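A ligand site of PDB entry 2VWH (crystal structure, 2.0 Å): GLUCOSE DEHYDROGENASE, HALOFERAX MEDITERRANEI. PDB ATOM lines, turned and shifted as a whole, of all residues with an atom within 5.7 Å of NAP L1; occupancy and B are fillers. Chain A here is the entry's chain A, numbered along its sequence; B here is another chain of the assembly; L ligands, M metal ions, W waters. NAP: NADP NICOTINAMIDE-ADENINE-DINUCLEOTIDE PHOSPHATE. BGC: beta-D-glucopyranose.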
ATOM      1  N   ASP A  38      26.106  22.072   6.396  1.00  0.00           N
ATOM      2  CA  ASP A  38      25.368  22.937   7.314  1.00  0.00           C
ATOM      3  C   ASP A  38      25.966  24.343   7.397  1.00  0.00           C
ATOM      4  O   ASP A  38      26.899  24.671   6.664  1.00  0.00           O
ATOM      5  CB  ASP A  38      25.137  22.272   8.694  1.00  0.00           C
ATOM      6  CG  ASP A  38      26.352  22.319   9.626  1.00  0.00           C
ATOM      7  OD1 ASP A  38      27.453  22.761   9.272  1.00  0.00           O
ATOM      8  OD2 ASP A  38      26.178  21.884  10.775  1.00  0.00           O
ATOM      9  N   GLY A  39      25.392  25.176   8.246  1.00  0.00           N
ATOM     10  CA  GLY A  39      25.837  26.561   8.405  1.00  0.00           C
ATOM     11  C   GLY A  39      27.262  26.669   8.914  1.00  0.00           C
ATOM     12  O   GLY A  39      27.959  27.607   8.572  1.00  0.00           O
ATOM     13  N   THR A  40      27.698  25.708   9.732  1.00  0.00           N
ATOM     14  CA  THR A  40      29.097  25.688  10.202  1.00  0.00           C
ATOM     15  C   THR A  40      30.074  25.476   9.031  1.00  0.00           C
ATOM     16  O   THR A  40      31.113  26.127   8.962  1.00  0.00           O
ATOM     17  CB  THR A  40      29.291  24.626  11.312  1.00  0.00           C
ATOM     18  OG1 THR A  40      28.396  24.905  12.410  1.00  0.00           O
ATOM     19  CG2 THR A  40      30.733  24.611  11.818  1.00  0.00           C
ATOM     20  N   HIS A  63      31.380  17.164   7.807  1.00  0.00           N
ATOM     21  CA  HIS A  63      31.367  16.524   9.125  1.00  0.00           C
ATOM     22  C   HIS A  63      30.099  15.701   9.412  1.00  0.00           C
ATOM     23  O   HIS A  63      30.082  14.951  10.385  1.00  0.00           O
ATOM     24  CB  HIS A  63      31.618  17.569  10.233  1.00  0.00           C
ATOM     25  CG  HIS A  63      30.546  18.600  10.355  1.00  0.00           C
ATOM     26  ND1 HIS A  63      30.548  19.759   9.617  1.00  0.00           N
ATOM     27  CD2 HIS A  63      29.445  18.657  11.146  1.00  0.00           C
ATOM     28  CE1 HIS A  63      29.486  20.484   9.947  1.00  0.00           C
ATOM     29  NE2 HIS A  63      28.804  19.835  10.869  1.00  0.00           N
ATOM     30  N   GLU A 150      23.965  13.063  12.661  1.00  0.00           N
ATOM     31  CA  GLU A 150      24.842  13.996  13.373  1.00  0.00           C
ATOM     32  C   GLU A 150      24.122  15.239  13.908  1.00  0.00           C
ATOM     33  O   GLU A 150      24.220  15.525  15.105  1.00  0.00           O
ATOM     34  CB  GLU A 150      26.090  14.339  12.539  1.00  0.00           C
ATOM     35  CG  GLU A 150      27.215  15.010  13.334  1.00  0.00           C
ATOM     36  CD  GLU A 150      27.099  16.514  13.424  1.00  0.00           C
ATOM     37  OE1 GLU A 150      26.215  17.080  12.752  1.00  0.00           O
ATOM     38  OE2 GLU A 150      27.906  17.127  14.166  1.00  0.00           O
ATOM     39  N   ILE A 154      23.323  16.524  17.965  1.00  0.00           N
ATOM     40  CA  ILE A 154      23.621  17.801  18.566  1.00  0.00           C
ATOM     41  C   ILE A 154      22.492  18.213  19.527  1.00  0.00           C
ATOM     42  O   ILE A 154      22.734  18.569  20.687  1.00  0.00           O
ATOM     43  CB  ILE A 154      23.803  18.905  17.489  1.00  0.00           C
ATOM     44  CG1 ILE A 154      25.008  18.614  16.576  1.00  0.00           C
ATOM     45  CG2 ILE A 154      23.913  20.309  18.141  1.00  0.00           C
ATOM     46  CD1 ILE A 154      26.383  18.583  17.274  1.00  0.00           C
ATOM     47  N   LEU A 179      14.873  29.501  18.089  1.00  0.00           N
ATOM     48  CA  LEU A 179      15.355  30.707  17.425  1.00  0.00           C
ATOM     49  C   LEU A 179      16.194  30.257  16.241  1.00  0.00           C
ATOM     50  O   LEU A 179      17.243  29.637  16.417  1.00  0.00           O
ATOM     51  CB  LEU A 179      16.176  31.570  18.366  1.00  0.00           C
ATOM     52  CG  LEU A 179      15.611  31.816  19.750  1.00  0.00           C
ATOM     53  CD1 LEU A 179      16.541  32.749  20.520  1.00  0.00           C
ATOM     54  CD2 LEU A 179      14.200  32.387  19.679  1.00  0.00           C
ATOM     55  N   GLY A 180      15.696  30.546  15.039  1.00  0.00           N
ATOM     56  CA  GLY A 180      16.396  30.180  13.810  1.00  0.00           C
ATOM     57  C   GLY A 180      15.652  29.168  12.973  1.00  0.00           C
ATOM     58  O   GLY A 180      15.089  28.204  13.491  1.00  0.00           O
ATOM     59  N   ASN A 181      15.660  29.403  11.665  1.00  0.00           N
ATOM     60  CA  ASN A 181      14.920  28.595  10.707  1.00  0.00           C
ATOM     61  C   ASN A 181      15.873  27.968   9.688  1.00  0.00           C
ATOM     62  O   ASN A 181      15.506  27.762   8.522  1.00  0.00           O
ATOM     63  CB  ASN A 181      13.844  29.442  10.002  1.00  0.00           C
ATOM     64  CG  ASN A 181      14.414  30.646   9.255  1.00  0.00           C
ATOM     65  OD1 ASN A 181      15.373  31.258   9.705  1.00  0.00           O
ATOM     66  ND2 ASN A 181      13.832  30.965   8.094  1.00  0.00           N
ATOM     67  N   GLY A 182      17.086  27.674  10.141  1.00  0.00           N
ATOM     68  CA  GLY A 182      18.053  26.910   9.378  1.00  0.00           C
ATOM     69  C   GLY A 182      17.787  25.427   9.584  1.00  0.00           C
ATOM     70  O   GLY A 182      16.798  25.039  10.206  1.00  0.00           O
ATOM     71  N   SER A 183      18.677  24.593   9.043  1.00  0.00           N
ATOM     72  CA  SER A 183      18.476  23.155   9.132  1.00  0.00           C
ATOM     73  C   SER A 183      18.515  22.655  10.599  1.00  0.00           C
ATOM     74  O   SER A 183      17.718  21.775  10.963  1.00  0.00           O
ATOM     75  CB  SER A 183      19.471  22.408   8.222  1.00  0.00           C
ATOM     76  OG  SER A 183      20.800  22.678   8.592  1.00  0.00           O
ATOM     77  N   LEU A 184      19.379  23.229  11.442  1.00  0.00           N
ATOM     78  CA  LEU A 184      19.385  22.828  12.869  1.00  0.00           C
ATOM     79  C   LEU A 184      18.094  23.239  13.592  1.00  0.00           C
ATOM     80  O   LEU A 184      17.487  22.437  14.303  1.00  0.00           O
ATOM     81  CB  LEU A 184      20.600  23.391  13.617  1.00  0.00           C
ATOM     82  CG  LEU A 184      20.809  22.881  15.049  1.00  0.00           C
ATOM     83  CD1 LEU A 184      20.979  21.371  15.093  1.00  0.00           C
ATOM     84  CD2 LEU A 184      22.013  23.564  15.705  1.00  0.00           C
ATOM     85  N   GLY A 185      17.674  24.485  13.407  1.00  0.00           N
ATOM     86  CA  GLY A 185      16.447  24.986  14.020  1.00  0.00           C
ATOM     87  C   GLY A 185      15.220  24.188  13.605  1.00  0.00           C
ATOM     88  O   GLY A 185      14.403  23.804  14.452  1.00  0.00           O
ATOM     89  N   LEU A 205      11.433  31.323  15.324  1.00  0.00           N
ATOM     90  CA  LEU A 205      11.836  32.659  14.868  1.00  0.00           C
ATOM     91  C   LEU A 205      12.627  32.620  13.572  1.00  0.00           C
ATOM     92  O   LEU A 205      13.555  31.806  13.413  1.00  0.00           O
ATOM     93  CB  LEU A 205      12.722  33.306  15.929  1.00  0.00           C
ATOM     94  CG  LEU A 205      13.079  34.774  15.761  1.00  0.00           C
ATOM     95  CD1 LEU A 205      12.081  35.654  16.467  1.00  0.00           C
ATOM     96  CD2 LEU A 205      14.460  35.020  16.302  1.00  0.00           C
ATOM     97  N   GLY A 206      12.279  33.528  12.678  1.00  0.00           N
ATOM     98  CA  GLY A 206      12.988  33.694  11.407  1.00  0.00           C
ATOM     99  C   GLY A 206      12.808  35.126  10.955  1.00  0.00           C
ATOM    100  O   GLY A 206      12.256  35.934  11.683  1.00  0.00           O
ATOM    101  N   ARG A 207      13.254  35.447   9.744  1.00  0.00           N
ATOM    102  CA  ARG A 207      13.116  36.799   9.209  1.00  0.00           C
ATOM    103  C   ARG A 207      12.855  36.784   7.694  1.00  0.00           C
ATOM    104  O   ARG A 207      13.504  37.500   6.943  1.00  0.00           O
ATOM    105  CB  ARG A 207      14.356  37.623   9.550  1.00  0.00           C
ATOM    106  CG  ARG A 207      15.681  37.019   9.089  1.00  0.00           C
ATOM    107  CD  ARG A 207      16.857  37.868   9.502  1.00  0.00           C
ATOM    108  NE  ARG A 207      18.107  37.304   9.025  1.00  0.00           N
ATOM    109  CZ  ARG A 207      19.322  37.727   9.376  1.00  0.00           C
ATOM    110  NH1 ARG A 207      19.483  38.728  10.221  1.00  0.00           N
ATOM    111  NH2 ARG A 207      20.391  37.130   8.864  1.00  0.00           N
ATOM    112  N   ARG A 208      11.905  35.952   7.263  1.00  0.00           N
ATOM    113  CA  ARG A 208      11.607  35.729   5.842  1.00  0.00           C
ATOM    114  C   ARG A 208      10.240  36.321   5.484  1.00  0.00           C
ATOM    115  O   ARG A 208       9.331  36.312   6.310  1.00  0.00           O
ATOM    116  CB  ARG A 208      11.565  34.246   5.517  1.00  0.00           C
ATOM    117  CG  ARG A 208      12.843  33.470   5.796  1.00  0.00           C
ATOM    118  CD  ARG A 208      13.944  33.869   4.832  1.00  0.00           C
ATOM    119  NE  ARG A 208      15.177  33.131   5.072  1.00  0.00           N
ATOM    120  CZ  ARG A 208      15.422  31.887   4.659  1.00  0.00           C
ATOM    121  NH1 ARG A 208      14.522  31.200   3.962  1.00  0.00           N
ATOM    122  NH2 ARG A 208      16.577  31.319   4.945  1.00  0.00           N
ATOM    123  N   SER A 228      11.219  38.079  13.336  1.00  0.00           N
ATOM    124  CA  SER A 228      12.006  38.923  14.266  1.00  0.00           C
ATOM    125  C   SER A 228      12.040  40.405  13.851  1.00  0.00           C
ATOM    126  O   SER A 228      12.317  41.265  14.690  1.00  0.00           O
ATOM    127  CB  SER A 228      13.431  38.411  14.422  1.00  0.00           C
ATOM    128  OG  SER A 228      14.180  38.555  13.228  1.00  0.00           O
ATOM    129  N   ALA A 249      19.489  28.862  17.828  1.00  0.00           N
ATOM    130  CA  ALA A 249      20.206  28.304  16.672  1.00  0.00           C
ATOM    131  C   ALA A 249      20.375  29.346  15.564  1.00  0.00           C
ATOM    132  O   ALA A 249      20.278  29.013  14.361  1.00  0.00           O
ATOM    133  CB  ALA A 249      19.482  27.071  16.162  1.00  0.00           C
ATOM    134  N   THR A 250      20.640  30.598  15.955  1.00  0.00           N
ATOM    135  CA  THR A 250      20.865  31.691  14.994  1.00  0.00           C
ATOM    136  C   THR A 250      22.319  32.117  14.895  1.00  0.00           C
ATOM    137  O   THR A 250      22.726  32.634  13.855  1.00  0.00           O
ATOM    138  CB  THR A 250      20.053  32.969  15.336  1.00  0.00           C
ATOM    139  OG1 THR A 250      20.410  33.471  16.636  1.00  0.00           O
ATOM    140  CG2 THR A 250      18.583  32.698  15.288  1.00  0.00           C
ATOM    141  N   GLY A 251      23.091  31.958  15.962  1.00  0.00           N
ATOM    142  CA  GLY A 251      24.443  32.512  16.022  1.00  0.00           C
ATOM    143  C   GLY A 251      24.473  34.025  16.179  1.00  0.00           C
ATOM    144  O   GLY A 251      25.522  34.637  16.007  1.00  0.00           O
ATOM    145  N   PHE A 252      23.339  34.635  16.513  1.00  0.00           N
ATOM    146  CA  PHE A 252      23.227  36.083  16.717  1.00  0.00           C
ATOM    147  C   PHE A 252      23.275  36.422  18.219  1.00  0.00           C
ATOM    148  O   PHE A 252      22.340  36.137  18.949  1.00  0.00           O
ATOM    149  CB  PHE A 252      21.900  36.563  16.096  1.00  0.00           C
ATOM    150  CG  PHE A 252      21.727  38.055  16.090  1.00  0.00           C
ATOM    151  CD1 PHE A 252      22.751  38.900  15.683  1.00  0.00           C
ATOM    152  CD2 PHE A 252      20.515  38.620  16.468  1.00  0.00           C
ATOM    153  CE1 PHE A 252      22.567  40.281  15.662  1.00  0.00           C
ATOM    154  CE2 PHE A 252      20.319  39.994  16.451  1.00  0.00           C
ATOM    155  CZ  PHE A 252      21.349  40.818  16.050  1.00  0.00           C
ATOM    156  N   HIS A 255      20.450  37.429  20.677  1.00  0.00           N
ATOM    157  CA  HIS A 255      19.482  36.396  21.068  1.00  0.00           C
ATOM    158  C   HIS A 255      19.895  35.654  22.345  1.00  0.00           C
ATOM    159  O   HIS A 255      19.053  35.305  23.150  1.00  0.00           O
ATOM    160  CB  HIS A 255      19.259  35.400  19.930  1.00  0.00           C
ATOM    161  CG  HIS A 255      18.524  35.982  18.771  1.00  0.00           C
ATOM    162  ND1 HIS A 255      18.541  35.405  17.511  1.00  0.00           N
ATOM    163  CD2 HIS A 255      17.767  37.101  18.662  1.00  0.00           C
ATOM    164  CE1 HIS A 255      17.806  36.140  16.692  1.00  0.00           C
ATOM    165  NE2 HIS A 255      17.324  37.165  17.372  1.00  0.00           N
ATOM    166  N   LEU A 271      21.849  27.296  24.303  1.00  0.00           N
ATOM    167  CA  LEU A 271      22.546  28.096  23.297  1.00  0.00           C
ATOM    168  C   LEU A 271      23.443  27.186  22.484  1.00  0.00           C
ATOM    169  O   LEU A 271      24.270  26.456  23.027  1.00  0.00           O
ATOM    170  CB  LEU A 271      23.402  29.190  23.967  1.00  0.00           C
ATOM    171  CG  LEU A 271      22.674  30.093  24.967  1.00  0.00           C
ATOM    172  CD1 LEU A 271      23.694  31.040  25.607  1.00  0.00           C
ATOM    173  CD2 LEU A 271      21.522  30.855  24.287  1.00  0.00           C
ATOM    174  N   LEU A 272      23.234  27.199  21.166  1.00  0.00           N
ATOM    175  CA  LEU A 272      23.985  26.348  20.232  1.00  0.00           C
ATOM    176  C   LEU A 272      24.748  27.134  19.160  1.00  0.00           C
ATOM    177  O   LEU A 272      25.628  26.590  18.491  1.00  0.00           O
ATOM    178  CB  LEU A 272      23.023  25.407  19.489  1.00  0.00           C
ATOM    179  CG  LEU A 272      22.464  24.162  20.185  1.00  0.00           C
ATOM    180  CD1 LEU A 272      23.549  23.124  20.476  1.00  0.00           C
ATOM    181  CD2 LEU A 272      21.698  24.499  21.452  1.00  0.00           C
ATOM    182  N   GLY A 273      24.383  28.399  18.964  1.00  0.00           N
ATOM    183  CA  GLY A 273      24.915  29.155  17.841  1.00  0.00           C
ATOM    184  C   GLY A 273      26.390  29.441  17.968  1.00  0.00           C
ATOM    185  O   GLY A 273      26.889  29.708  19.067  1.00  0.00           O
ATOM    186  N   VAL A 274      27.096  29.401  16.840  1.00  0.00           N
ATOM    187  CA  VAL A 274      28.500  29.824  16.801  1.00  0.00           C
ATOM    188  C   VAL A 274      28.509  31.288  16.351  1.00  0.00           C
ATOM    189  O   VAL A 274      28.242  31.604  15.192  1.00  0.00           O
ATOM    190  CB  VAL A 274      29.337  28.947  15.866  1.00  0.00           C
ATOM    191  CG1 VAL A 274      30.776  29.456  15.784  1.00  0.00           C
ATOM    192  CG2 VAL A 274      29.307  27.478  16.351  1.00  0.00           C
ATOM    193  N   PRO A 275      28.768  32.191  17.305  1.00  0.00           N
ATOM    194  CA  PRO A 275      28.479  33.596  17.085  1.00  0.00           C
ATOM    195  C   PRO A 275      29.578  34.362  16.369  1.00  0.00           C
ATOM    196  O   PRO A 275      30.732  33.951  16.369  1.00  0.00           O
ATOM    197  CB  PRO A 275      28.347  34.123  18.511  1.00  0.00           C
ATOM    198  CG  PRO A 275      29.343  33.334  19.248  1.00  0.00           C
ATOM    199  CD  PRO A 275      29.332  31.959  18.639  1.00  0.00           C
ATOM    200  N   SER A 301      25.932  24.444  24.689  1.00  0.00           N
ATOM    201  CA  SER A 301      26.247  23.084  24.287  1.00  0.00           C
ATOM    202  C   SER A 301      26.956  23.049  22.934  1.00  0.00           C
ATOM    203  O   SER A 301      26.631  23.814  22.012  1.00  0.00           O
ATOM    204  CB  SER A 301      24.975  22.251  24.238  1.00  0.00           C
ATOM    205  OG  SER A 301      25.244  20.873  24.037  1.00  0.00           O
ATOM    206  N   VAL A 302      27.944  22.170  22.801  1.00  0.00           N
ATOM    207  CA  VAL A 302      28.626  21.984  21.524  1.00  0.00           C
ATOM    208  C   VAL A 302      28.959  20.523  21.302  1.00  0.00           C
ATOM    209  O   VAL A 302      29.241  19.790  22.261  1.00  0.00           O
ATOM    210  CB  VAL A 302      29.903  22.881  21.391  1.00  0.00           C
ATOM    211  CG1 VAL A 302      31.033  22.423  22.374  1.00  0.00           C
ATOM    212  CG2 VAL A 302      30.404  22.895  19.948  1.00  0.00           C
ATOM    213  N   ASN A 303      28.882  20.093  20.045  1.00  0.00           N
ATOM    214  CA  ASN A 303      29.304  18.751  19.657  1.00  0.00           C
ATOM    215  C   ASN A 303      28.364  17.719  20.278  1.00  0.00           C
ATOM    216  O   ASN A 303      27.253  18.059  20.710  1.00  0.00           O
ATOM    217  CB  ASN A 303      30.784  18.535  20.037  1.00  0.00           C
ATOM    218  CG  ASN A 303      31.428  17.352  19.330  1.00  0.00           C
ATOM    219  OD1 ASN A 303      31.838  16.391  19.982  1.00  0.00           O
ATOM    220  ND2 ASN A 303      31.499  17.389  18.007  1.00  0.00           N
ATOM    221  N   ASP A 343      23.220  28.921  -1.192  1.00  0.00           N
ATOM    222  CA  ASP A 343      22.668  29.362   0.082  1.00  0.00           C
ATOM    223  C   ASP A 343      21.586  30.406  -0.159  1.00  0.00           C
ATOM    224  O   ASP A 343      21.588  31.467   0.471  1.00  0.00           O
ATOM    225  CB  ASP A 343      23.792  29.900   0.986  1.00  0.00           C
ATOM    226  CG  ASP A 343      23.423  29.868   2.475  1.00  0.00           C
ATOM    227  OD1 ASP A 343      22.385  29.276   2.831  1.00  0.00           O
ATOM    228  OD2 ASP A 343      24.185  30.448   3.285  1.00  0.00           O
ATOM    229  N   ASP A 345      17.329  31.378  -0.173  1.00  0.00           N
ATOM    230  CA  ASP A 345      16.221  31.161   0.753  1.00  0.00           C
ATOM    231  C   ASP A 345      15.481  29.835   0.552  1.00  0.00           C
ATOM    232  O   ASP A 345      14.933  29.292   1.509  1.00  0.00           O
ATOM    233  CB  ASP A 345      15.215  32.311   0.638  1.00  0.00           C
ATOM    234  CG  ASP A 345      15.731  33.615   1.241  1.00  0.00           C
ATOM    235  OD1 ASP A 345      16.846  33.638   1.810  1.00  0.00           O
ATOM    236  OD2 ASP A 345      14.993  34.614   1.171  1.00  0.00           O
ATOM    237  N   VAL B 292      28.761  28.662  24.516  1.00  0.00           N
ATOM    238  CA  VAL B 292      28.547  27.558  23.594  1.00  0.00           C
ATOM    239  C   VAL B 292      29.778  26.670  23.471  1.00  0.00           C
ATOM    240  O   VAL B 292      29.730  25.460  23.765  1.00  0.00           O
ATOM    241  CB  VAL B 292      28.095  28.070  22.197  1.00  0.00           C
ATOM    242  CG1 VAL B 292      28.023  26.931  21.187  1.00  0.00           C
ATOM    243  CG2 VAL B 292      26.724  28.765  22.314  1.00  0.00           C
HETATM  244  PA  NAP L   1      22.085  28.343   9.297  1.00  0.00           P
HETATM  245  O1A NAP L   1      21.682  27.529   8.127  1.00  0.00           O
HETATM  246  O2A NAP L   1      22.971  29.458   9.036  1.00  0.00           O
HETATM  247  O5B NAP L   1      20.758  28.829  10.031  1.00  0.00           O
HETATM  248  C5B NAP L   1      20.757  30.008  10.812  1.00  0.00           C
HETATM  249  C4B NAP L   1      19.420  30.673  10.586  1.00  0.00           C
HETATM  250  O4B NAP L   1      19.244  31.704  11.529  1.00  0.00           O
HETATM  251  C3B NAP L   1      19.325  31.294   9.190  1.00  0.00           C
HETATM  252  O3B NAP L   1      18.300  30.659   8.457  1.00  0.00           O
HETATM  253  C2B NAP L   1      19.034  32.754   9.461  1.00  0.00           C
HETATM  254  O2B NAP L   1      18.042  33.267   8.615  1.00  0.00           O
HETATM  255  C1B NAP L   1      18.545  32.747  10.900  1.00  0.00           C
HETATM  256  N9A NAP L   1      18.778  34.057  11.529  1.00  0.00           N
HETATM  257  C8A NAP L   1      19.988  34.710  11.676  1.00  0.00           C
HETATM  258  N7A NAP L   1      19.757  35.883  12.291  1.00  0.00           N
HETATM  259  C5A NAP L   1      18.421  35.996  12.515  1.00  0.00           C
HETATM  260  C6A NAP L   1      17.666  36.995  13.104  1.00  0.00           C
HETATM  261  N6A NAP L   1      18.251  38.097  13.565  1.00  0.00           N
HETATM  262  N1A NAP L   1      16.303  36.826  13.213  1.00  0.00           N
HETATM  263  C2A NAP L   1      15.697  35.664  12.752  1.00  0.00           C
HETATM  264  N3A NAP L   1      16.464  34.675  12.169  1.00  0.00           N
HETATM  265  C4A NAP L   1      17.797  34.847  12.052  1.00  0.00           C
HETATM  266  O3  NAP L   1      22.802  27.364  10.358  1.00  0.00           O
HETATM  267  PN  NAP L   1      22.391  25.914  10.917  1.00  0.00           P
HETATM  268  O1N NAP L   1      20.919  25.805  11.081  1.00  0.00           O
HETATM  269  O2N NAP L   1      23.129  24.855  10.181  1.00  0.00           O
HETATM  270  O5D NAP L   1      23.044  26.066  12.379  1.00  0.00           O
HETATM  271  C5D NAP L   1      22.590  27.031  13.299  1.00  0.00           C
HETATM  272  C4D NAP L   1      23.722  27.624  14.120  1.00  0.00           C
HETATM  273  O4D NAP L   1      24.236  26.633  14.983  1.00  0.00           O
HETATM  274  C3D NAP L   1      24.933  28.136  13.350  1.00  0.00           C
HETATM  275  O3D NAP L   1      25.511  29.210  14.065  1.00  0.00           O
HETATM  276  C2D NAP L   1      25.855  26.942  13.329  1.00  0.00           C
HETATM  277  O2D NAP L   1      27.199  27.248  13.112  1.00  0.00           O
HETATM  278  C1D NAP L   1      25.629  26.401  14.730  1.00  0.00           C
HETATM  279  N1N NAP L   1      25.860  24.960  14.967  1.00  0.00           N
HETATM  280  C2N NAP L   1      26.415  24.644  16.182  1.00  0.00           C
HETATM  281  C3N NAP L   1      26.615  23.333  16.559  1.00  0.00           C
HETATM  282  C7N NAP L   1      27.013  23.066  17.986  1.00  0.00           C
HETATM  283  O7N NAP L   1      27.567  21.808  18.267  1.00  0.00           O
HETATM  284  N7N NAP L   1      26.858  23.985  18.955  1.00  0.00           N
HETATM  285  C4N NAP L   1      26.265  22.309  15.677  1.00  0.00           C
HETATM  286  C5N NAP L   1      25.654  22.651  14.448  1.00  0.00           C
HETATM  287  C6N NAP L   1      25.458  23.982  14.096  1.00  0.00           C
HETATM  288  P2B NAP L   1      18.406  33.948   7.196  1.00  0.00           P
HETATM  289  O1X NAP L   1      18.733  32.862   6.234  1.00  0.00           O
HETATM  290  O2X NAP L   1      19.558  34.880   7.340  1.00  0.00           O
HETATM  291  O3X NAP L   1      17.154  34.672   6.782  1.00  0.00           O
HETATM  292  C2  BGC L   2      29.276  20.269  14.257  1.00  0.00           C
HETATM  293  C3  BGC L   2      29.696  19.908  15.670  1.00  0.00           C
HETATM  294  C4  BGC L   2      30.766  20.891  16.102  1.00  0.00           C
HETATM  295  C5  BGC L   2      30.256  22.349  15.951  1.00  0.00           C
HETATM  296  C6  BGC L   2      31.348  23.340  16.388  1.00  0.00           C
HETATM  297  C1  BGC L   2      28.827  21.713  14.189  1.00  0.00           C
HETATM  298  O1  BGC L   2      28.291  21.927  12.910  1.00  0.00           O
HETATM  299  O2  BGC L   2      28.092  19.568  13.986  1.00  0.00           O
HETATM  300  O3  BGC L   2      30.186  18.575  15.707  1.00  0.00           O
HETATM  301  O4  BGC L   2      31.203  20.583  17.401  1.00  0.00           O
HETATM  302  O5  BGC L   2      29.837  22.601  14.595  1.00  0.00           O
HETATM  303  O6  BGC L   2      32.381  23.275  15.448  1.00  0.00           O
HETATM  304 ZN    ZN M   1      27.257  20.559  11.862  1.00  0.00          ZN
HETATM  305  O   HOH W   1      16.664  40.029  15.493  1.00  0.00           O
HETATM  306  O   HOH W   2      18.932  27.191  12.448  1.00  0.00           O
HETATM  307  O   HOH W   3      15.085  33.711   8.467  1.00  0.00           O
HETATM  308  O   HOH W   4      24.850  31.324  12.194  1.00  0.00           O
HETATM  309  O   HOH W   5      27.886  29.897  12.431  1.00  0.00           O
HETATM  310  O   HOH W   6      17.036  36.829   5.340  1.00  0.00           O
HETATM  311  O   HOH W   7      23.402  22.351  11.544  1.00  0.00           O
HETATM  312  O   HOH W   8      19.501  28.991   6.564  1.00  0.00           O
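Residues that only touch NAP L1: Ala 249, Gly 182, Val 302, Gly 206, Ile 154, Asp 38, His 255, Phe 252, Leu 205, Gly 273, Thr 250, Val 292 of chain B, Gly 180 and Gly 251. Hydrophobic or aromatic side chains within 4 Å of NAP L1: Ile 154, Leu 184, Leu 205, Phe 252, His 255, Leu 272, Val 274, Val 302 and Val 292 of chain B. Within 4 Å of NAP L1: Asp 38, Gly 39, Thr 40, Ile 154, Gly 180, Asn 181, Gly 182, Ser 183, Leu 184, Leu 205, Gly 206, Arg 207, Arg 208, Ser 228, Ala 249, Thr 250, Gly 251, Phe 252, His 255, Leu 272, Gly 273, Val 274, Ser 301, Val 302, Asn 303 and Val 292 of chain B. The nearest printed residue that does not touch NAP L1 is Gly 185 (4.2 Å).
The side-chain hydroxyl (OG1) of Thr 40 sits at hydrogen-bond distance from an oxygen (O2D) of NAP L1, 2.7 Å away. The side-chain hydroxyl of Ser 228 sits at hydrogen-bond distance from a nitrogen (N1A) of NAP L1, at 2.7 Å. N of Asn 303 is in hydrogen-bond range of O7N of NAP L1. An oxygen (O2X) of NAP L1 is in salt-bridge range of the guanidinium group (NH2) of Arg 207 (2.8 Å). The backbone carbonyl oxygen (O) of Leu 272 sits at hydrogen-bond distance from a nitrogen (N7N) of NAP L1, 2.9 Å away. The guanidinium group (NH2) of Arg 208 is in salt-bridge range of an oxygen (O1X) of NAP L1, at 2.9 Å. N of Gly 39 lies within hydrogen-bond range of O2N of NAP L1 (3.0 Å). O1N of NAP L1 sits at hydrogen-bond distance from N of Leu 184 (3.0 Å). The backbone carbonyl oxygen of Ser 301 is in hydrogen-bond range of a nitrogen (N7N) of NAP L1 (3.1 Å). An oxygen (O3D) of NAP L1 lies within hydrogen-bond range of the backbone NH (N) of Val 274 (3.2 Å). An oxygen (O3B) of NAP L1 lies within hydrogen-bond range of the side-chain amide oxygen (OD1) of Asn 181 (3.2 Å). O1N of NAP L1 is in hydrogen-bond range of N of Ser 183 (3.3 Å). OG1 of Thr 40 is in hydrogen-bond range of O5 of BGC L2. O3 of BGC L2 is in hydrogen-bond range of ND2 of Asn 303 (2.9 Å). The side-chain carboxylate of Glu 150 is in hydrogen-bond range of an oxygen (O3) of BGC L2, at 3.1 Å.
Water W2 lies within hydrogen-bond range of O1N of NAP L1 (2.8 Å), O of Ala 249 (3.0 Å), N of Gly 182 (3.0 Å) and N of Gly 185 (3.1 Å). Water W5 lies within hydrogen-bond range of O2D of NAP L1 and O of Val 274. Water W3 lies within hydrogen-bond range of OD1 of Asn 181 (2.8 Å), N of Arg 207 (2.8 Å), O3X of NAP L1 (2.8 Å) and NE of Arg 208 (3.4 Å). Water W4 lies within hydrogen-bond range of an oxygen (O3D) of NAP L1 (2.9 Å) and the backbone carbonyl oxygen (O) of Thr 250 (3.0 Å). Water W1 bridges N6A of NAP L1 (3.2 Å) and NE2 of His 255 (3.5 Å).
The backbone NH of Thr 40 is in hydrogen-bond range of the side-chain carboxylate of Asp 38 (3.0 Å). The backbone NH (N) of Ser 228 lies within hydrogen-bond range of the backbone carbonyl oxygen (O) of Gly 206, at 2.9 Å. The guanidinium group (NE) of Arg 208 is in salt-bridge range of the side-chain carboxylate (OD1) of Asp 345, 3.7 Å away. O of Leu 271 sits at hydrogen-bond distance from N of Ser 301, at 3.1 Å. The backbone carbonyl oxygen (O) of Leu 179 lies within hydrogen-bond range of the backbone NH (N) of Ala 249. The side-chain hydroxyl of Thr 250 sits at hydrogen-bond distance from a ring nitrogen (ND1) of His 255, 2.8 Å away. OG1 of Thr 250 lies within hydrogen-bond range of N of Phe 252. The backbone carbonyl oxygen (O) of Leu 205 is in hydrogen-bond range of the backbone NH (N) of Gly 180 (3.0 Å).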
